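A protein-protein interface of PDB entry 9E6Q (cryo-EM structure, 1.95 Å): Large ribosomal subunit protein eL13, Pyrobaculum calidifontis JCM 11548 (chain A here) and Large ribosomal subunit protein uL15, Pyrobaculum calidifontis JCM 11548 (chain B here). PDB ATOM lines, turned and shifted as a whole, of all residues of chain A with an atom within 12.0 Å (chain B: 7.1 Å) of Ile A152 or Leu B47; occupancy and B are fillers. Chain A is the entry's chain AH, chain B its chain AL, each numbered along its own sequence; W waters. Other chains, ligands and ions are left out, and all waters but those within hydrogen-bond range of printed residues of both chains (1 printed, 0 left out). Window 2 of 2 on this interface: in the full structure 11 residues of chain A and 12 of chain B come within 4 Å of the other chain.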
ATOM      1  N   GLY A 143     -12.939   9.892 -13.823  1.00  0.00           N
ATOM      2  CA  GLY A 143     -11.934   9.773 -14.864  1.00  0.00           C
ATOM      3  C   GLY A 143     -10.521   9.981 -14.354  1.00  0.00           C
ATOM      4  O   GLY A 143      -9.594   9.292 -14.779  1.00  0.00           O
ATOM      5  N   ASN A 144     -10.334  10.943 -13.455  1.00  0.00           N
ATOM      6  CA  ASN A 144      -8.994  11.216 -12.948  1.00  0.00           C
ATOM      7  C   ASN A 144      -8.536  10.164 -11.948  1.00  0.00           C
ATOM      8  O   ASN A 144      -7.342   9.870 -11.870  1.00  0.00           O
ATOM      9  CB  ASN A 144      -8.942  12.604 -12.320  1.00  0.00           C
ATOM     10  CG  ASN A 144      -7.659  13.327 -12.632  1.00  0.00           C
ATOM     11  OD1 ASN A 144      -6.969  12.997 -13.586  1.00  0.00           O
ATOM     12  ND2 ASN A 144      -7.326  14.312 -11.822  1.00  0.00           N
ATOM     13  N   VAL A 145      -9.456   9.599 -11.170  1.00  0.00           N
ATOM     14  CA  VAL A 145      -9.092   8.503 -10.280  1.00  0.00           C
ATOM     15  C   VAL A 145      -8.643   7.294 -11.088  1.00  0.00           C
ATOM     16  O   VAL A 145      -7.660   6.632 -10.745  1.00  0.00           O
ATOM     17  CB  VAL A 145     -10.266   8.159  -9.346  1.00  0.00           C
ATOM     18  CG1 VAL A 145      -9.966   6.907  -8.560  1.00  0.00           C
ATOM     19  CG2 VAL A 145     -10.548   9.314  -8.415  1.00  0.00           C
ATOM     20  N   LEU A 146      -9.358   6.984 -12.171  1.00  0.00           N
ATOM     21  CA  LEU A 146      -8.942   5.904 -13.059  1.00  0.00           C
ATOM     22  C   LEU A 146      -7.597   6.197 -13.705  1.00  0.00           C
ATOM     23  O   LEU A 146      -6.736   5.317 -13.781  1.00  0.00           O
ATOM     24  CB  LEU A 146      -9.994   5.683 -14.139  1.00  0.00           C
ATOM     25  CG  LEU A 146     -11.240   4.889 -13.767  1.00  0.00           C
ATOM     26  CD1 LEU A 146     -12.335   5.165 -14.764  1.00  0.00           C
ATOM     27  CD2 LEU A 146     -10.927   3.417 -13.709  1.00  0.00           C
ATOM     28  N   ARG A 147      -7.400   7.428 -14.182  1.00  0.00           N
ATOM     29  CA  ARG A 147      -6.172   7.778 -14.885  1.00  0.00           C
ATOM     30  C   ARG A 147      -4.949   7.630 -13.988  1.00  0.00           C
ATOM     31  O   ARG A 147      -3.951   7.022 -14.381  1.00  0.00           O
ATOM     32  CB  ARG A 147      -6.271   9.208 -15.419  1.00  0.00           C
ATOM     33  CG  ARG A 147      -5.162   9.590 -16.362  1.00  0.00           C
ATOM     34  CD  ARG A 147      -5.144  11.075 -16.668  1.00  0.00           C
ATOM     35  NE  ARG A 147      -4.935  11.914 -15.494  1.00  0.00           N
ATOM     36  CZ  ARG A 147      -3.802  12.545 -15.225  1.00  0.00           C
ATOM     37  NH1 ARG A 147      -2.736  12.403 -15.989  1.00  0.00           N
ATOM     38  NH2 ARG A 147      -3.733  13.328 -14.157  1.00  0.00           N
ATOM     39  N   ILE A 148      -5.007   8.184 -12.778  1.00  0.00           N
ATOM     40  CA  ILE A 148      -3.862   8.103 -11.879  1.00  0.00           C
ATOM     41  C   ILE A 148      -3.637   6.676 -11.414  1.00  0.00           C
ATOM     42  O   ILE A 148      -2.494   6.239 -11.266  1.00  0.00           O
ATOM     43  CB  ILE A 148      -4.041   9.064 -10.691  1.00  0.00           C
ATOM     44  CG1 ILE A 148      -4.082  10.509 -11.184  1.00  0.00           C
ATOM     45  CG2 ILE A 148      -2.942   8.866  -9.662  1.00  0.00           C
ATOM     46  CD1 ILE A 148      -2.772  11.020 -11.663  1.00  0.00           C
ATOM     47  N   SER A 149      -4.711   5.924 -11.181  1.00  0.00           N
ATOM     48  CA  SER A 149      -4.563   4.550 -10.715  1.00  0.00           C
ATOM     49  C   SER A 149      -3.971   3.656 -11.794  1.00  0.00           C
ATOM     50  O   SER A 149      -3.204   2.738 -11.489  1.00  0.00           O
ATOM     51  CB  SER A 149      -5.907   4.006 -10.243  1.00  0.00           C
ATOM     52  OG  SER A 149      -6.505   3.214 -11.249  1.00  0.00           O
ATOM     53  N   ARG A 150      -4.328   3.892 -13.057  1.00  0.00           N
ATOM     54  CA  ARG A 150      -3.747   3.116 -14.146  1.00  0.00           C
ATOM     55  C   ARG A 150      -2.248   3.339 -14.247  1.00  0.00           C
ATOM     56  O   ARG A 150      -1.489   2.394 -14.469  1.00  0.00           O
ATOM     57  CB  ARG A 150      -4.424   3.465 -15.468  1.00  0.00           C
ATOM     58  CG  ARG A 150      -5.789   2.844 -15.659  1.00  0.00           C
ATOM     59  CD  ARG A 150      -6.242   2.953 -17.100  1.00  0.00           C
ATOM     60  NE  ARG A 150      -6.029   4.289 -17.642  1.00  0.00           N
ATOM     61  CZ  ARG A 150      -6.992   5.178 -17.841  1.00  0.00           C
ATOM     62  NH1 ARG A 150      -8.257   4.897 -17.577  1.00  0.00           N
ATOM     63  NH2 ARG A 150      -6.678   6.379 -18.312  1.00  0.00           N
ATOM     64  N   ILE A 151      -1.800   4.584 -14.089  1.00  0.00           N
ATOM     65  CA  ILE A 151      -0.373   4.875 -14.155  1.00  0.00           C
ATOM     66  C   ILE A 151       0.374   4.128 -13.061  1.00  0.00           C
ATOM     67  O   ILE A 151       1.426   3.528 -13.299  1.00  0.00           O
ATOM     68  CB  ILE A 151      -0.127   6.390 -14.053  1.00  0.00           C
ATOM     69  CG1 ILE A 151      -0.706   7.122 -15.260  1.00  0.00           C
ATOM     70  CG2 ILE A 151       1.344   6.663 -13.923  1.00  0.00           C
ATOM     71  CD1 ILE A 151      -0.820   8.603 -15.054  1.00  0.00           C
ATOM     72  N   ILE A 152      -0.160   4.157 -11.842  1.00  0.00           N
ATOM     73  CA  ILE A 152       0.525   3.530 -10.720  1.00  0.00           C
ATOM     74  C   ILE A 152       0.527   2.014 -10.864  1.00  0.00           C
ATOM     75  O   ILE A 152       1.536   1.355 -10.595  1.00  0.00           O
ATOM     76  CB  ILE A 152      -0.115   3.978  -9.397  1.00  0.00           C
ATOM     77  CG1 ILE A 152       0.146   5.464  -9.167  1.00  0.00           C
ATOM     78  CG2 ILE A 152       0.418   3.162  -8.243  1.00  0.00           C
ATOM     79  CD1 ILE A 152      -0.661   6.050  -8.057  1.00  0.00           C
ATOM     80  N   ASN A 153      -0.585   1.437 -11.297  1.00  0.00           N
ATOM     81  CA  ASN A 153      -0.692  -0.011 -11.352  1.00  0.00           C
ATOM     82  C   ASN A 153      -0.187  -0.607 -12.657  1.00  0.00           C
ATOM     83  O   ASN A 153      -0.088  -1.831 -12.756  1.00  0.00           O
ATOM     84  CB  ASN A 153      -2.142  -0.432 -11.111  1.00  0.00           C
ATOM     85  CG  ASN A 153      -2.628  -0.048  -9.731  1.00  0.00           C
ATOM     86  OD1 ASN A 153      -1.964  -0.313  -8.736  1.00  0.00           O
ATOM     87  ND2 ASN A 153      -3.776   0.601  -9.669  1.00  0.00           N
ATOM     88  N   GLU A 154       0.137   0.211 -13.653  1.00  0.00           N
ATOM     89  CA  GLU A 154       0.674  -0.278 -14.916  1.00  0.00           C
ATOM     90  C   GLU A 154       2.094   0.201 -15.168  1.00  0.00           C
ATOM     91  O   GLU A 154       2.589   0.069 -16.289  1.00  0.00           O
ATOM     92  CB  GLU A 154      -0.221   0.146 -16.080  1.00  0.00           C
ATOM     93  CG  GLU A 154      -1.534  -0.602 -16.171  1.00  0.00           C
ATOM     94  CD  GLU A 154      -2.528   0.083 -17.088  1.00  0.00           C
ATOM     95  OE1 GLU A 154      -3.729   0.104 -16.750  1.00  0.00           O
ATOM     96  OE2 GLU A 154      -2.108   0.608 -18.140  1.00  0.00           O
ATOM     97  N   SER A 155       2.753   0.765 -14.166  1.00  0.00           N
ATOM     98  CA  SER A 155       4.091   1.310 -14.346  1.00  0.00           C
ATOM     99  C   SER A 155       5.101   0.202 -14.598  1.00  0.00           C
ATOM    100  O   SER A 155       5.182  -0.752 -13.831  1.00  0.00           O
ATOM    101  CB  SER A 155       4.506   2.130 -13.125  1.00  0.00           C
ATOM    102  OG  SER A 155       5.421   3.147 -13.483  1.00  0.00           O
ATOM    103  N   PHE B  40       0.421  16.430  -6.882  1.00  0.00           N
ATOM    104  CA  PHE B  40       1.418  15.591  -7.527  1.00  0.00           C
ATOM    105  C   PHE B  40       2.597  16.368  -8.083  1.00  0.00           C
ATOM    106  O   PHE B  40       3.577  15.744  -8.488  1.00  0.00           O
ATOM    107  CB  PHE B  40       0.767  14.768  -8.630  1.00  0.00           C
ATOM    108  CG  PHE B  40      -0.087  13.668  -8.111  1.00  0.00           C
ATOM    109  CD1 PHE B  40       0.477  12.593  -7.464  1.00  0.00           C
ATOM    110  CD2 PHE B  40      -1.456  13.714  -8.248  1.00  0.00           C
ATOM    111  CE1 PHE B  40      -0.308  11.584  -6.971  1.00  0.00           C
ATOM    112  CE2 PHE B  40      -2.238  12.711  -7.762  1.00  0.00           C
ATOM    113  CZ  PHE B  40      -1.664  11.646  -7.118  1.00  0.00           C
ATOM    114  N   HIS B  43       4.017  18.233  -3.233  1.00  0.00           N
ATOM    115  CA  HIS B  43       4.419  17.394  -2.114  1.00  0.00           C
ATOM    116  C   HIS B  43       4.262  15.914  -2.397  1.00  0.00           C
ATOM    117  O   HIS B  43       4.822  15.100  -1.663  1.00  0.00           O
ATOM    118  CB  HIS B  43       3.659  17.762  -0.831  1.00  0.00           C
ATOM    119  CG  HIS B  43       2.178  17.895  -0.995  1.00  0.00           C
ATOM    120  ND1 HIS B  43       1.592  18.965  -1.630  1.00  0.00           N
ATOM    121  CD2 HIS B  43       1.162  17.112  -0.567  1.00  0.00           C
ATOM    122  CE1 HIS B  43       0.282  18.820  -1.614  1.00  0.00           C
ATOM    123  NE2 HIS B  43      -0.005  17.708  -0.968  1.00  0.00           N
ATOM    124  N   LYS B  44       3.542  15.550  -3.450  1.00  0.00           N
ATOM    125  CA  LYS B  44       3.491  14.178  -3.927  1.00  0.00           C
ATOM    126  C   LYS B  44       4.293  13.991  -5.207  1.00  0.00           C
ATOM    127  O   LYS B  44       4.101  13.004  -5.913  1.00  0.00           O
ATOM    128  CB  LYS B  44       2.040  13.747  -4.118  1.00  0.00           C
ATOM    129  CG  LYS B  44       1.219  13.929  -2.865  1.00  0.00           C
ATOM    130  CD  LYS B  44      -0.166  13.363  -2.994  1.00  0.00           C
ATOM    131  CE  LYS B  44      -1.001  13.749  -1.794  1.00  0.00           C
ATOM    132  NZ  LYS B  44      -2.427  13.390  -1.970  1.00  0.00           N
ATOM    133  N   TRP B  45       5.180  14.934  -5.520  1.00  0.00           N
ATOM    134  CA  TRP B  45       6.095  14.799  -6.647  1.00  0.00           C
ATOM    135  C   TRP B  45       7.011  13.598  -6.487  1.00  0.00           C
ATOM    136  O   TRP B  45       7.470  13.036  -7.482  1.00  0.00           O
ATOM    137  CB  TRP B  45       6.903  16.087  -6.786  1.00  0.00           C
ATOM    138  CG  TRP B  45       7.892  16.168  -7.920  1.00  0.00           C
ATOM    139  CD1 TRP B  45       9.237  16.292  -7.809  1.00  0.00           C
ATOM    140  CD2 TRP B  45       7.604  16.189  -9.323  1.00  0.00           C
ATOM    141  NE1 TRP B  45       9.812  16.374  -9.046  1.00  0.00           N
ATOM    142  CE2 TRP B  45       8.830  16.313  -9.995  1.00  0.00           C
ATOM    143  CE3 TRP B  45       6.431  16.107 -10.075  1.00  0.00           C
ATOM    144  CZ2 TRP B  45       8.917  16.362 -11.378  1.00  0.00           C
ATOM    145  CZ3 TRP B  45       6.523  16.147 -11.448  1.00  0.00           C
ATOM    146  CH2 TRP B  45       7.754  16.270 -12.086  1.00  0.00           C
ATOM    147  N   SER B  46       7.284  13.186  -5.250  1.00  0.00           N
ATOM    148  CA  SER B  46       8.085  11.990  -5.024  1.00  0.00           C
ATOM    149  C   SER B  46       7.345  10.734  -5.450  1.00  0.00           C
ATOM    150  O   SER B  46       7.973   9.713  -5.736  1.00  0.00           O
ATOM    151  CB  SER B  46       8.478  11.896  -3.556  1.00  0.00           C
ATOM    152  OG  SER B  46       7.345  12.059  -2.736  1.00  0.00           O
ATOM    153  N   LEU B  47       6.018  10.784  -5.486  1.00  0.00           N
ATOM    154  CA  LEU B  47       5.251   9.674  -6.027  1.00  0.00           C
ATOM    155  C   LEU B  47       5.304   9.654  -7.548  1.00  0.00           C
ATOM    156  O   LEU B  47       5.281   8.584  -8.160  1.00  0.00           O
ATOM    157  CB  LEU B  47       3.812   9.759  -5.540  1.00  0.00           C
ATOM    158  CG  LEU B  47       2.975   8.494  -5.658  1.00  0.00           C
ATOM    159  CD1 LEU B  47       2.102   8.356  -4.449  1.00  0.00           C
ATOM    160  CD2 LEU B  47       2.134   8.542  -6.915  1.00  0.00           C
ATOM    161  N   VAL B  48       5.338  10.828  -8.177  1.00  0.00           N
ATOM    162  CA  VAL B  48       5.493  10.891  -9.626  1.00  0.00           C
ATOM    163  C   VAL B  48       6.858  10.360 -10.039  1.00  0.00           C
ATOM    164  O   VAL B  48       6.983   9.621 -11.017  1.00  0.00           O
ATOM    165  CB  VAL B  48       5.273  12.331 -10.124  1.00  0.00           C
ATOM    166  CG1 VAL B  48       5.595  12.440 -11.595  1.00  0.00           C
ATOM    167  CG2 VAL B  48       3.859  12.777  -9.853  1.00  0.00           C
ATOM    168  N   MET B  49       7.903  10.732  -9.304  1.00  0.00           N
ATOM    169  CA  MET B  49       9.247  10.283  -9.639  1.00  0.00           C
ATOM    170  C   MET B  49       9.402   8.777  -9.475  1.00  0.00           C
ATOM    171  O   MET B  49      10.207   8.162 -10.175  1.00  0.00           O
ATOM    172  CB  MET B  49      10.260  11.040  -8.786  1.00  0.00           C
ATOM    173  CG  MET B  49      10.676  12.398  -9.348  1.00  0.00           C
ATOM    174  SD  MET B  49      10.967  12.405 -11.127  1.00  0.00           S
ATOM    175  CE  MET B  49       9.461  13.107 -11.758  1.00  0.00           C
ATOM    176  N   LYS B  50       8.643   8.167  -8.564  1.00  0.00           N
ATOM    177  CA  LYS B  50       8.716   6.722  -8.383  1.00  0.00           C
ATOM    178  C   LYS B  50       8.115   5.973  -9.565  1.00  0.00           C
ATOM    179  O   LYS B  50       8.702   5.002 -10.049  1.00  0.00           O
ATOM    180  CB  LYS B  50       8.006   6.314  -7.093  1.00  0.00           C
ATOM    181  CG  LYS B  50       7.861   4.812  -6.931  1.00  0.00           C
ATOM    182  CD  LYS B  50       7.133   4.445  -5.663  1.00  0.00           C
ATOM    183  CE  LYS B  50       7.036   2.945  -5.513  1.00  0.00           C
ATOM    184  NZ  LYS B  50       6.114   2.559  -4.425  1.00  0.00           N
ATOM    185  N   TYR B  51       6.953   6.404 -10.044  1.00  0.00           N
ATOM    186  CA  TYR B  51       6.230   5.676 -11.075  1.00  0.00           C
ATOM    187  C   TYR B  51       6.360   6.271 -12.466  1.00  0.00           C
ATOM    188  O   TYR B  51       6.173   5.547 -13.446  1.00  0.00           O
ATOM    189  CB  TYR B  51       4.743   5.609 -10.730  1.00  0.00           C
ATOM    190  CG  TYR B  51       4.443   4.770  -9.530  1.00  0.00           C
ATOM    191  CD1 TYR B  51       4.573   3.397  -9.577  1.00  0.00           C
ATOM    192  CD2 TYR B  51       4.035   5.348  -8.344  1.00  0.00           C
ATOM    193  CE1 TYR B  51       4.296   2.623  -8.484  1.00  0.00           C
ATOM    194  CE2 TYR B  51       3.755   4.579  -7.242  1.00  0.00           C
ATOM    195  CZ  TYR B  51       3.888   3.216  -7.319  1.00  0.00           C
ATOM    196  OH  TYR B  51       3.609   2.442  -6.222  1.00  0.00           O
ATOM    197  N   GLY B  52       6.647   7.564 -12.584  1.00  0.00           N
ATOM    198  CA  GLY B  52       6.642   8.233 -13.862  1.00  0.00           C
ATOM    199  C   GLY B  52       8.032   8.436 -14.436  1.00  0.00           C
ATOM    200  O   GLY B  52       9.046   8.038 -13.873  1.00  0.00           O
ATOM    201  N   PHE B  60       1.919  11.352 -15.625  1.00  0.00           N
ATOM    202  CA  PHE B  60       1.111  12.156 -14.717  1.00  0.00           C
ATOM    203  C   PHE B  60       0.785  13.518 -15.319  1.00  0.00           C
ATOM    204  O   PHE B  60      -0.331  14.016 -15.153  1.00  0.00           O
ATOM    205  CB  PHE B  60       1.823  12.320 -13.376  1.00  0.00           C
ATOM    206  CG  PHE B  60       1.857  11.073 -12.544  1.00  0.00           C
ATOM    207  CD1 PHE B  60       2.819  10.106 -12.756  1.00  0.00           C
ATOM    208  CD2 PHE B  60       0.932  10.877 -11.536  1.00  0.00           C
ATOM    209  CE1 PHE B  60       2.856   8.971 -11.983  1.00  0.00           C
ATOM    210  CE2 PHE B  60       0.962   9.739 -10.766  1.00  0.00           C
ATOM    211  CZ  PHE B  60       1.923   8.784 -10.990  1.00  0.00           C
HETATM  212  O   HOH W   1       4.671   5.194 -15.718  1.00  0.00           O
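CG2 of Ile A148 touches CZ of Phe B40 (3.98 Å).
CD2 of Phe B60 touches CD1 of Ile A148, at 3.7 Å.
CG2 of Ile A151 touches CE1 of Phe B60, 3.4 Å away.
Ile A152 touches Leu B47 (CD1 to CD2, 3.9 Å).
Tyr B51 touches Ile A152.
Gly A143 touches none of the printed residues of chain B.
Val A145 touches none of the printed residues of chain B.
Of the printed residues of chain B, Arg A147 touches Phe B60 (3.0 Å).
Of the printed residues of chain B, Ile A148 touches Phe B40 and Phe B60.
Of the printed residues of chain B, Ile A151 touches Phe B60.
Of chain B, only Leu B47 (3.9 Å) and Tyr B51 (3.6 Å) come within 4 Å of Ile A152.
Of the printed residues of chain B, Ser A155 touches Tyr B51.
Of chain A, only Ile A148 (3.98 Å) comes within 4 Å of Phe B40.
Of chain A, only Ile A152 comes within 4 Å of Leu B47.
No residue of chain A comes within 4 Å of Val B48.
No residue of chain A comes within 4 Å of Met B49.
Tyr B51 touches two residues of chain A.
No residue of chain A comes within 4 Å of Gly B52.
Printed residues of chain A within 4 Å of Phe B60: Arg A147, Ile A148 and Ile A151.
The nearest residue of chain B that does not touch Ile A152 is Phe B60 (4.2 Å).
The nearest printed residue of chain B that does not touch Ile A151 is Tyr B51 (4.7 Å).
Of the 12 printed residues of chain B, 4 touch a printed residue of chain A.
Printed residues of chain B that touch a printed residue of chain A: Phe B40, Leu B47, Tyr B51 and Phe B60.
Hydrophobic or aromatic side chains of chain B within 4 Å of the printed part of chain A: Phe B40, Leu B47, Tyr B51 and Phe B60.
Hydrophobic or aromatic side chains of chain A that line the printed part of chain B: Ile A148, Ile A151 and Ile A152.
Among the printed residues, 7 pairs touch across the chains.
Among the printed residues, no Asp or Glu carboxylate lies within 4 Å of a Lys or Arg side-chain nitrogen of the other chain.
The guanidinium group (NE) of Arg A147 sits at hydrogen-bond distance from the side-chain amide oxygen (OD1) of Asn A144.
N of Trp B45 sits close to O of Phe B40 (3.5 Å).
The side-chain amino group (NZ) of Lys B50 sits at hydrogen-bond distance from the side-chain hydroxyl (OH) of Tyr B51, 3.1 Å away.
Water W1 lies within hydrogen-bond range of O of Tyr B51 and OG of Ser A155.
NH1 of Arg A147 is in hydrogen-bond range of O of Phe B60 (3.0 Å).
The backbone carbonyl oxygen (O) of Tyr B51 is in hydrogen-bond range of the side-chain hydroxyl (OG) of Ser A155, at 2.5 Å.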
